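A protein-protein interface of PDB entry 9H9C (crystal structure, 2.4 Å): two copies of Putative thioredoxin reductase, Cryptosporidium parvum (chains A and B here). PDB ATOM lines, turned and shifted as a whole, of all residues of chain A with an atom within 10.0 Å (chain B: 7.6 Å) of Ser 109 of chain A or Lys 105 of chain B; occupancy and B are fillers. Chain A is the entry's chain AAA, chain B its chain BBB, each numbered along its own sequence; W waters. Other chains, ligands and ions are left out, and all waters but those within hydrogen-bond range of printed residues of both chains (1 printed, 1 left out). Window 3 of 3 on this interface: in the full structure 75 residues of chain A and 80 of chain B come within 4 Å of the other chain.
N of Glu 111 of chain A is in hydrogen-bond range of O of Gly 103 of chain B (2.8 Å). The backbone carbonyl oxygen (O) of Gly 103 of chain B sits close to the backbone carbonyl oxygen (O) of Ser 109 of chain A, 3.5 Å away. The side-chain hydroxyl (OG) of Ser 88 of chain A sits at hydrogen-bond distance from a ring nitrogen (NE2) of His 104 of chain B, at 3.0 Å. The backbone NH (N) of Ser 109 of chain A sits at hydrogen-bond distance from the backbone carbonyl oxygen (O) of Lys 105 of chain B (3.2 Å). The backbone carbonyl oxygen of Phe 102 of chain B lies within hydrogen-bond range of the side-chain hydroxyl of Ser 88 of chain A (2.6 Å). N of Ser 107 of chain A lies within hydrogen-bond range of O of Ser 107 of chain B (3.0 Å).
O of Ala 99 of chain B lies within hydrogen-bond range of N of His 104 of chain B (2.7 Å).
Among the printed residues, merely in contact across the chains: Ser 107 of chain A with Thr 106 of chain B (3.3 Å), Phe 110 of chain A with Gly 103 of chain B (3.3 Å), Thr 106 of chain A with Ser 107 of chain B (3.3 Å), Ser 108 of chain A with Lys 105 of chain B (3.3 Å), Phe 110 of chain A with His 104 of chain B (3.4 Å), Ser 108 of chain A with Thr 106 of chain B (3.5 Å), Lys 114 of chain A with Gln 100 of chain B (3.5 Å), Ala 92 of chain A with His 104 of chain B (3.6 Å), Leu 226 of chain A with His 104 of chain B (3.6 Å), Ile 95 of chain A with Thr 106 of chain B (3.6 Å), Leu 115 of chain A with Phe 102 of chain B (3.7 Å), Ser 109 of chain A with His 104 of chain B (3.7 Å), Thr 106 of chain A with Ile 95 of chain B (3.8 Å), Phe 110 of chain A with Phe 102 of chain B (3.9 Å), Ser 108 of chain A with His 104 of chain B (3.9 Å), Lys 114 of chain A with Gly 103 of chain B (3.95 Å), Ile 91 of chain A with His 104 of chain B (3.99 Å) and Ser 107 of chain A with Lys 105 of chain B (3.99 Å).
Of the printed residues of chain B, Ile 95 of chain A touches Thr 106 (3.6 Å). Printed residues of chain B within 4 Å of Ser 108 of chain A: His 104 (3.9 Å), Lys 105 (3.3 Å) and Thr 106 (3.5 Å). Of chain B, only Gly 103, His 104 and Lys 105 come within 4 Å of Ser 109 of chain A. Gly 113 of chain A touches none of the printed residues of chain B. Met 101 of chain B touches none of the printed residues of chain A. Gly 103 of chain B touches four residues of chain A. Printed residues of chain A within 4 Å of His 104 of chain B: Ser 88 (3.0 Å), Ile 91 (3.99 Å), Ala 92 (3.6 Å), Ser 108 (3.9 Å), Ser 109 (3.7 Å), Phe 110 (3.4 Å) and Leu 226 (3.6 Å). Printed residues of chain A within 4 Å of Lys 105 of chain B: Ser 107, Ser 108 and Ser 109. Of chain A, only Ile 95, Ser 107 and Ser 108 come within 4 Å of Thr 106 of chain B.
Hydrophobic or aromatic side chains of chain A within 4 Å of the printed part of chain B: Ile 91, Ala 92, Ile 95, Phe 110, Leu 115 and Leu 226. Of the 10 printed residues of chain B, 8 touch a printed residue of chain A. Hydrophobic or aromatic side chains of chain B that line the printed part of chain A: Ile 95, Phe 102 and His 104. Along chain B the printed residues that touch a printed residue of chain A span positions 95 to 107.
Ile 95 of chain A touches Thr 106 of chain B, and with the chains exchanged Thr 106 of chain A touches Ile 95 of chain B. Thr 106 of chain A touches Ser 107 of chain B, and with the chains exchanged Ser 107 of chain A touches Thr 106 of chain B. Ser 107 of chain A touches its own counterpart, Ser 107 of chain B. 3 positions are printed for both chains.
Water W1 lies within hydrogen-bond range of O of Ser 109 of chain A, O of Gly 103 of chain B and N of Lys 105 of chain B.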
ATOM      1  N   SER A  88      18.699 -22.229   9.419  1.00  0.00           N
ATOM      2  CA  SER A  88      18.387 -22.469   7.992  1.00  0.00           C
ATOM      3  C   SER A  88      19.519 -21.945   7.128  1.00  0.00           C
ATOM      4  O   SER A  88      19.851 -22.615   6.155  1.00  0.00           O
ATOM      5  CB  SER A  88      17.084 -21.824   7.564  1.00  0.00           C
ATOM      6  OG  SER A  88      16.761 -22.171   6.217  1.00  0.00           O
ATOM      7  N   ILE A  91      22.560 -24.043   7.325  1.00  0.00           N
ATOM      8  CA  ILE A  91      22.293 -25.290   6.562  1.00  0.00           C
ATOM      9  C   ILE A  91      22.567 -24.994   5.079  1.00  0.00           C
ATOM     10  O   ILE A  91      23.319 -25.786   4.458  1.00  0.00           O
ATOM     11  CB  ILE A  91      20.873 -25.836   6.813  1.00  0.00           C
ATOM     12  CG1 ILE A  91      20.750 -26.367   8.235  1.00  0.00           C
ATOM     13  CG2 ILE A  91      20.540 -26.907   5.771  1.00  0.00           C
ATOM     14  CD1 ILE A  91      19.409 -26.964   8.533  1.00  0.00           C
ATOM     15  N   ALA A  92      21.983 -23.918   4.540  1.00  0.00           N
ATOM     16  CA  ALA A  92      22.257 -23.446   3.160  1.00  0.00           C
ATOM     17  C   ALA A  92      23.774 -23.399   2.904  1.00  0.00           C
ATOM     18  O   ALA A  92      24.250 -24.012   1.918  1.00  0.00           O
ATOM     19  CB  ALA A  92      21.646 -22.080   2.965  1.00  0.00           C
ATOM     20  N   ILE A  95      25.506 -26.770   2.831  1.00  0.00           N
ATOM     21  CA  ILE A  95      25.125 -27.506   1.593  1.00  0.00           C
ATOM     22  C   ILE A  95      25.858 -26.899   0.390  1.00  0.00           C
ATOM     23  O   ILE A  95      26.403 -27.674  -0.389  1.00  0.00           O
ATOM     24  CB  ILE A  95      23.616 -27.492   1.346  1.00  0.00           C
ATOM     25  CG1 ILE A  95      22.862 -28.347   2.359  1.00  0.00           C
ATOM     26  CG2 ILE A  95      23.312 -27.951  -0.083  1.00  0.00           C
ATOM     27  CD1 ILE A  95      21.351 -28.279   2.219  1.00  0.00           C
ATOM     28  N   HIS A  96      25.874 -25.573   0.235  1.00  0.00           N
ATOM     29  CA  HIS A  96      26.605 -24.896  -0.876  1.00  0.00           C
ATOM     30  C   HIS A  96      28.112 -25.178  -0.790  1.00  0.00           C
ATOM     31  O   HIS A  96      28.672 -25.676  -1.800  1.00  0.00           O
ATOM     32  CB  HIS A  96      26.342 -23.394  -0.913  1.00  0.00           C
ATOM     33  CG  HIS A  96      27.018 -22.712  -2.061  1.00  0.00           C
ATOM     34  ND1 HIS A  96      28.119 -21.842  -1.880  1.00  0.00           N
ATOM     35  CD2 HIS A  96      26.787 -22.765  -3.396  1.00  0.00           C
ATOM     36  CE1 HIS A  96      28.532 -21.404  -3.056  1.00  0.00           C
ATOM     37  NE2 HIS A  96      27.749 -21.990  -4.011  1.00  0.00           N
ATOM     38  N   THR A 106      24.860 -33.283  -3.482  1.00  0.00           N
ATOM     39  CA  THR A 106      23.483 -32.867  -3.125  1.00  0.00           C
ATOM     40  C   THR A 106      22.875 -32.014  -4.232  1.00  0.00           C
ATOM     41  O   THR A 106      23.612 -31.241  -4.849  1.00  0.00           O
ATOM     42  CB  THR A 106      23.480 -32.040  -1.837  1.00  0.00           C
ATOM     43  OG1 THR A 106      24.068 -30.808  -2.218  1.00  0.00           O
ATOM     44  CG2 THR A 106      24.239 -32.671  -0.691  1.00  0.00           C
ATOM     45  N   SER A 107      21.571 -32.129  -4.447  1.00  0.00           N
ATOM     46  CA  SER A 107      20.778 -31.064  -5.103  1.00  0.00           C
ATOM     47  C   SER A 107      19.774 -30.563  -4.074  1.00  0.00           C
ATOM     48  O   SER A 107      19.288 -31.362  -3.267  1.00  0.00           O
ATOM     49  CB  SER A 107      20.137 -31.540  -6.386  1.00  0.00           C
ATOM     50  OG  SER A 107      19.320 -32.676  -6.172  1.00  0.00           O
ATOM     51  N   SER A 108      19.516 -29.273  -4.098  1.00  0.00           N
ATOM     52  CA  SER A 108      18.764 -28.555  -3.053  1.00  0.00           C
ATOM     53  C   SER A 108      18.002 -27.419  -3.717  1.00  0.00           C
ATOM     54  O   SER A 108      18.575 -26.803  -4.632  1.00  0.00           O
ATOM     55  CB  SER A 108      19.717 -28.013  -1.996  1.00  0.00           C
ATOM     56  OG  SER A 108      19.003 -27.464  -0.906  1.00  0.00           O
ATOM     57  N   SER A 109      16.795 -27.113  -3.244  1.00  0.00           N
ATOM     58  CA  SER A 109      16.129 -25.821  -3.544  1.00  0.00           C
ATOM     59  C   SER A 109      15.483 -25.307  -2.261  1.00  0.00           C
ATOM     60  O   SER A 109      14.990 -26.150  -1.453  1.00  0.00           O
ATOM     61  CB  SER A 109      15.128 -25.924  -4.685  1.00  0.00           C
ATOM     62  OG  SER A 109      14.273 -27.045  -4.540  1.00  0.00           O
ATOM     63  N   PHE A 110      15.458 -23.987  -2.109  1.00  0.00           N
ATOM     64  CA  PHE A 110      14.960 -23.305  -0.883  1.00  0.00           C
ATOM     65  C   PHE A 110      13.496 -22.924  -1.066  1.00  0.00           C
ATOM     66  O   PHE A 110      13.185 -22.375  -2.120  1.00  0.00           O
ATOM     67  CB  PHE A 110      15.772 -22.050  -0.570  1.00  0.00           C
ATOM     68  CG  PHE A 110      15.231 -21.329   0.626  1.00  0.00           C
ATOM     69  CD1 PHE A 110      15.189 -21.955   1.856  1.00  0.00           C
ATOM     70  CD2 PHE A 110      14.715 -20.050   0.508  1.00  0.00           C
ATOM     71  CE1 PHE A 110      14.695 -21.294   2.978  1.00  0.00           C
ATOM     72  CE2 PHE A 110      14.212 -19.386   1.624  1.00  0.00           C
ATOM     73  CZ  PHE A 110      14.197 -20.012   2.861  1.00  0.00           C
ATOM     74  N   GLU A 111      12.654 -23.182  -0.071  1.00  0.00           N
ATOM     75  CA  GLU A 111      11.233 -22.810  -0.099  1.00  0.00           C
ATOM     76  C   GLU A 111      10.926 -21.962   1.141  1.00  0.00           C
ATOM     77  O   GLU A 111      10.806 -22.531   2.228  1.00  0.00           O
ATOM     78  CB  GLU A 111      10.398 -24.089  -0.286  1.00  0.00           C
ATOM     79  CG  GLU A 111      10.575 -24.711  -1.681  1.00  0.00           C
ATOM     80  CD  GLU A 111      10.161 -23.868  -2.913  1.00  0.00           C
ATOM     81  OE1 GLU A 111      10.506 -24.290  -4.071  1.00  0.00           O
ATOM     82  OE2 GLU A 111       9.469 -22.769  -2.754  1.00  0.00           O
ATOM     83  N   TRP A 112      10.790 -20.655   0.954  1.00  0.00           N
ATOM     84  CA  TRP A 112      10.620 -19.646   2.040  1.00  0.00           C
ATOM     85  C   TRP A 112       9.456 -20.059   2.951  1.00  0.00           C
ATOM     86  O   TRP A 112       9.642 -20.068   4.201  1.00  0.00           O
ATOM     87  CB  TRP A 112      10.459 -18.225   1.468  1.00  0.00           C
ATOM     88  CG  TRP A 112      10.032 -17.195   2.480  1.00  0.00           C
ATOM     89  CD1 TRP A 112       8.756 -16.761   2.734  1.00  0.00           C
ATOM     90  CD2 TRP A 112      10.885 -16.477   3.400  1.00  0.00           C
ATOM     91  NE1 TRP A 112       8.770 -15.817   3.733  1.00  0.00           N
ATOM     92  CE2 TRP A 112      10.051 -15.633   4.163  1.00  0.00           C
ATOM     93  CE3 TRP A 112      12.265 -16.472   3.658  1.00  0.00           C
ATOM     94  CZ2 TRP A 112      10.545 -14.784   5.142  1.00  0.00           C
ATOM     95  CZ3 TRP A 112      12.756 -15.633   4.632  1.00  0.00           C
ATOM     96  CH2 TRP A 112      11.899 -14.827   5.386  1.00  0.00           C
ATOM     97  N   GLY A 113       8.305 -20.397   2.358  1.00  0.00           N
ATOM     98  CA  GLY A 113       7.054 -20.706   3.095  1.00  0.00           C
ATOM     99  C   GLY A 113       7.177 -21.935   4.002  1.00  0.00           C
ATOM    100  O   GLY A 113       6.457 -22.021   4.991  1.00  0.00           O
ATOM    101  N   LYS A 114       8.033 -22.884   3.649  1.00  0.00           N
ATOM    102  CA  LYS A 114       8.256 -24.104   4.460  1.00  0.00           C
ATOM    103  C   LYS A 114       8.986 -23.727   5.764  1.00  0.00           C
ATOM    104  O   LYS A 114       8.577 -24.218   6.829  1.00  0.00           O
ATOM    105  CB  LYS A 114       9.036 -25.122   3.631  1.00  0.00           C
ATOM    106  CG  LYS A 114       9.303 -26.433   4.343  1.00  0.00           C
ATOM    107  CD  LYS A 114       8.097 -26.999   5.073  1.00  0.00           C
ATOM    108  CE  LYS A 114       8.489 -28.290   5.744  1.00  0.00           C
ATOM    109  NZ  LYS A 114       7.316 -29.106   6.120  1.00  0.00           N
ATOM    110  N   LEU A 115      10.000 -22.861   5.675  1.00  0.00           N
ATOM    111  CA  LEU A 115      10.811 -22.374   6.828  1.00  0.00           C
ATOM    112  C   LEU A 115       9.910 -21.566   7.755  1.00  0.00           C
ATOM    113  O   LEU A 115       9.903 -21.820   8.972  1.00  0.00           O
ATOM    114  CB  LEU A 115      11.983 -21.528   6.317  1.00  0.00           C
ATOM    115  CG  LEU A 115      12.766 -20.779   7.386  1.00  0.00           C
ATOM    116  CD1 LEU A 115      13.408 -21.745   8.365  1.00  0.00           C
ATOM    117  CD2 LEU A 115      13.793 -19.843   6.761  1.00  0.00           C
ATOM    118  N   LEU A 226      20.514 -17.264   2.460  1.00  0.00           N
ATOM    119  CA  LEU A 226      19.329 -18.010   1.954  1.00  0.00           C
ATOM    120  C   LEU A 226      19.098 -17.725   0.467  1.00  0.00           C
ATOM    121  O   LEU A 226      18.066 -18.218  -0.076  1.00  0.00           O
ATOM    122  CB  LEU A 226      18.094 -17.633   2.773  1.00  0.00           C
ATOM    123  CG  LEU A 226      17.988 -18.265   4.160  1.00  0.00           C
ATOM    124  CD1 LEU A 226      16.764 -17.710   4.880  1.00  0.00           C
ATOM    125  CD2 LEU A 226      17.959 -19.788   4.084  1.00  0.00           C
ATOM    126  N   GLY A 227      19.991 -16.935  -0.150  1.00  0.00           N
ATOM    127  CA  GLY A 227      20.059 -16.743  -1.610  1.00  0.00           C
ATOM    128  C   GLY A 227      19.386 -15.466  -2.091  1.00  0.00           C
ATOM    129  O   GLY A 227      19.290 -15.291  -3.299  1.00  0.00           O
ATOM    130  N   PHE A 228      18.922 -14.589  -1.195  1.00  0.00           N
ATOM    131  CA  PHE A 228      18.228 -13.324  -1.579  1.00  0.00           C
ATOM    132  C   PHE A 228      19.261 -12.229  -1.870  1.00  0.00           C
ATOM    133  O   PHE A 228      20.299 -12.195  -1.191  1.00  0.00           O
ATOM    134  CB  PHE A 228      17.221 -12.935  -0.503  1.00  0.00           C
ATOM    135  CG  PHE A 228      16.134 -13.956  -0.342  1.00  0.00           C
ATOM    136  CD1 PHE A 228      15.229 -14.184  -1.359  1.00  0.00           C
ATOM    137  CD2 PHE A 228      16.039 -14.723   0.813  1.00  0.00           C
ATOM    138  CE1 PHE A 228      14.215 -15.118  -1.206  1.00  0.00           C
ATOM    139  CE2 PHE A 228      15.021 -15.650   0.970  1.00  0.00           C
ATOM    140  CZ  PHE A 228      14.125 -15.861  -0.049  1.00  0.00           C
ATOM    141  N   ILE B  95      21.293 -32.976   6.940  1.00  0.00           N
ATOM    142  CA  ILE B  95      20.601 -33.185   5.640  1.00  0.00           C
ATOM    143  C   ILE B  95      19.428 -34.147   5.825  1.00  0.00           C
ATOM    144  O   ILE B  95      18.363 -33.831   5.333  1.00  0.00           O
ATOM    145  CB  ILE B  95      21.551 -33.710   4.542  1.00  0.00           C
ATOM    146  CG1 ILE B  95      22.498 -32.611   4.068  1.00  0.00           C
ATOM    147  CG2 ILE B  95      20.753 -34.341   3.380  1.00  0.00           C
ATOM    148  CD1 ILE B  95      23.500 -33.072   3.050  1.00  0.00           C
ATOM    149  N   ALA B  99      17.235 -30.406   7.046  1.00  0.00           N
ATOM    150  CA  ALA B  99      17.308 -29.535   5.854  1.00  0.00           C
ATOM    151  C   ALA B  99      15.897 -29.222   5.352  1.00  0.00           C
ATOM    152  O   ALA B  99      15.575 -28.036   5.158  1.00  0.00           O
ATOM    153  CB  ALA B  99      18.142 -30.175   4.780  1.00  0.00           C
ATOM    154  N   GLN B 100      15.079 -30.250   5.142  1.00  0.00           N
ATOM    155  CA  GLN B 100      13.713 -30.088   4.593  1.00  0.00           C
ATOM    156  C   GLN B 100      12.895 -29.214   5.558  1.00  0.00           C
ATOM    157  O   GLN B 100      12.221 -28.265   5.084  1.00  0.00           O
ATOM    158  CB  GLN B 100      13.108 -31.460   4.293  1.00  0.00           C
ATOM    159  CG  GLN B 100      11.653 -31.400   3.865  1.00  0.00           C
ATOM    160  CD  GLN B 100      11.157 -32.729   3.306  1.00  0.00           C
ATOM    161  OE1 GLN B 100      11.815 -33.792   3.410  1.00  0.00           O
ATOM    162  NE2 GLN B 100       9.986 -32.672   2.663  1.00  0.00           N
ATOM    163  N   MET B 101      12.963 -29.492   6.855  1.00  0.00           N
ATOM    164  CA  MET B 101      12.189 -28.749   7.886  1.00  0.00           C
ATOM    165  C   MET B 101      12.523 -27.250   7.843  1.00  0.00           C
ATOM    166  O   MET B 101      11.635 -26.436   8.177  1.00  0.00           O
ATOM    167  CB  MET B 101      12.477 -29.288   9.297  1.00  0.00           C
ATOM    168  CG  MET B 101      11.793 -30.607   9.622  1.00  0.00           C
ATOM    169  SD  MET B 101       9.961 -30.413   9.527  1.00  0.00           S
ATOM    170  CE  MET B 101       9.617 -29.379  10.953  1.00  0.00           C
ATOM    171  N   PHE B 102      13.762 -26.898   7.523  1.00  0.00           N
ATOM    172  CA  PHE B 102      14.243 -25.500   7.517  1.00  0.00           C
ATOM    173  C   PHE B 102      14.197 -24.954   6.082  1.00  0.00           C
ATOM    174  O   PHE B 102      14.866 -23.945   5.811  1.00  0.00           O
ATOM    175  CB  PHE B 102      15.629 -25.387   8.183  1.00  0.00           C
ATOM    176  CG  PHE B 102      15.532 -25.462   9.672  1.00  0.00           C
ATOM    177  CD1 PHE B 102      15.427 -26.672  10.325  1.00  0.00           C
ATOM    178  CD2 PHE B 102      15.446 -24.297  10.418  1.00  0.00           C
ATOM    179  CE1 PHE B 102      15.202 -26.714  11.689  1.00  0.00           C
ATOM    180  CE2 PHE B 102      15.271 -24.358  11.799  1.00  0.00           C
ATOM    181  CZ  PHE B 102      15.156 -25.558  12.422  1.00  0.00           C
ATOM    182  N   GLY B 103      13.426 -25.610   5.206  1.00  0.00           N
ATOM    183  CA  GLY B 103      12.996 -25.106   3.885  1.00  0.00           C
ATOM    184  C   GLY B 103      13.894 -25.569   2.763  1.00  0.00           C
ATOM    185  O   GLY B 103      13.713 -25.093   1.609  1.00  0.00           O
ATOM    186  N   HIS B 104      14.874 -26.420   3.059  1.00  0.00           N
ATOM    187  CA  HIS B 104      15.855 -26.896   2.046  1.00  0.00           C
ATOM    188  C   HIS B 104      15.512 -28.332   1.676  1.00  0.00           C
ATOM    189  O   HIS B 104      15.982 -29.222   2.410  1.00  0.00           O
ATOM    190  CB  HIS B 104      17.291 -26.736   2.560  1.00  0.00           C
ATOM    191  CG  HIS B 104      17.645 -25.330   2.901  1.00  0.00           C
ATOM    192  ND1 HIS B 104      18.032 -24.417   1.938  1.00  0.00           N
ATOM    193  CD2 HIS B 104      17.675 -24.694   4.096  1.00  0.00           C
ATOM    194  CE1 HIS B 104      18.306 -23.266   2.517  1.00  0.00           C
ATOM    195  NE2 HIS B 104      18.070 -23.395   3.858  1.00  0.00           N
ATOM    196  N   LYS B 105      14.656 -28.544   0.662  1.00  0.00           N
ATOM    197  CA  LYS B 105      14.360 -29.908   0.127  1.00  0.00           C
ATOM    198  C   LYS B 105      15.606 -30.405  -0.628  1.00  0.00           C
ATOM    199  O   LYS B 105      16.027 -29.766  -1.610  1.00  0.00           O
ATOM    200  CB  LYS B 105      13.111 -29.951  -0.753  1.00  0.00           C
ATOM    201  CG  LYS B 105      12.725 -31.345  -1.240  1.00  0.00           C
ATOM    202  CD  LYS B 105      12.135 -32.241  -0.142  1.00  0.00           C
ATOM    203  CE  LYS B 105      12.186 -33.732  -0.425  1.00  0.00           C
ATOM    204  NZ  LYS B 105      11.287 -34.122  -1.550  1.00  0.00           N
ATOM    205  N   THR B 106      16.204 -31.480  -0.123  1.00  0.00           N
ATOM    206  CA  THR B 106      17.500 -31.994  -0.590  1.00  0.00           C
ATOM    207  C   THR B 106      17.396 -33.477  -0.941  1.00  0.00           C
ATOM    208  O   THR B 106      16.710 -34.221  -0.233  1.00  0.00           O
ATOM    209  CB  THR B 106      18.538 -31.831   0.510  1.00  0.00           C
ATOM    210  OG1 THR B 106      18.066 -32.735   1.512  1.00  0.00           O
ATOM    211  CG2 THR B 106      18.675 -30.409   0.986  1.00  0.00           C
ATOM    212  N   SER B 107      18.057 -33.883  -2.004  1.00  0.00           N
ATOM    213  CA  SER B 107      18.422 -35.310  -2.209  1.00  0.00           C
ATOM    214  C   SER B 107      19.937 -35.367  -2.227  1.00  0.00           C
ATOM    215  O   SER B 107      20.579 -34.401  -2.704  1.00  0.00           O
ATOM    216  CB  SER B 107      17.796 -35.939  -3.440  1.00  0.00           C
ATOM    217  OG  SER B 107      18.061 -35.177  -4.593  1.00  0.00           O
HETATM  218  O   HOH W   1      12.913 -26.707  -0.346  1.00  0.00           O
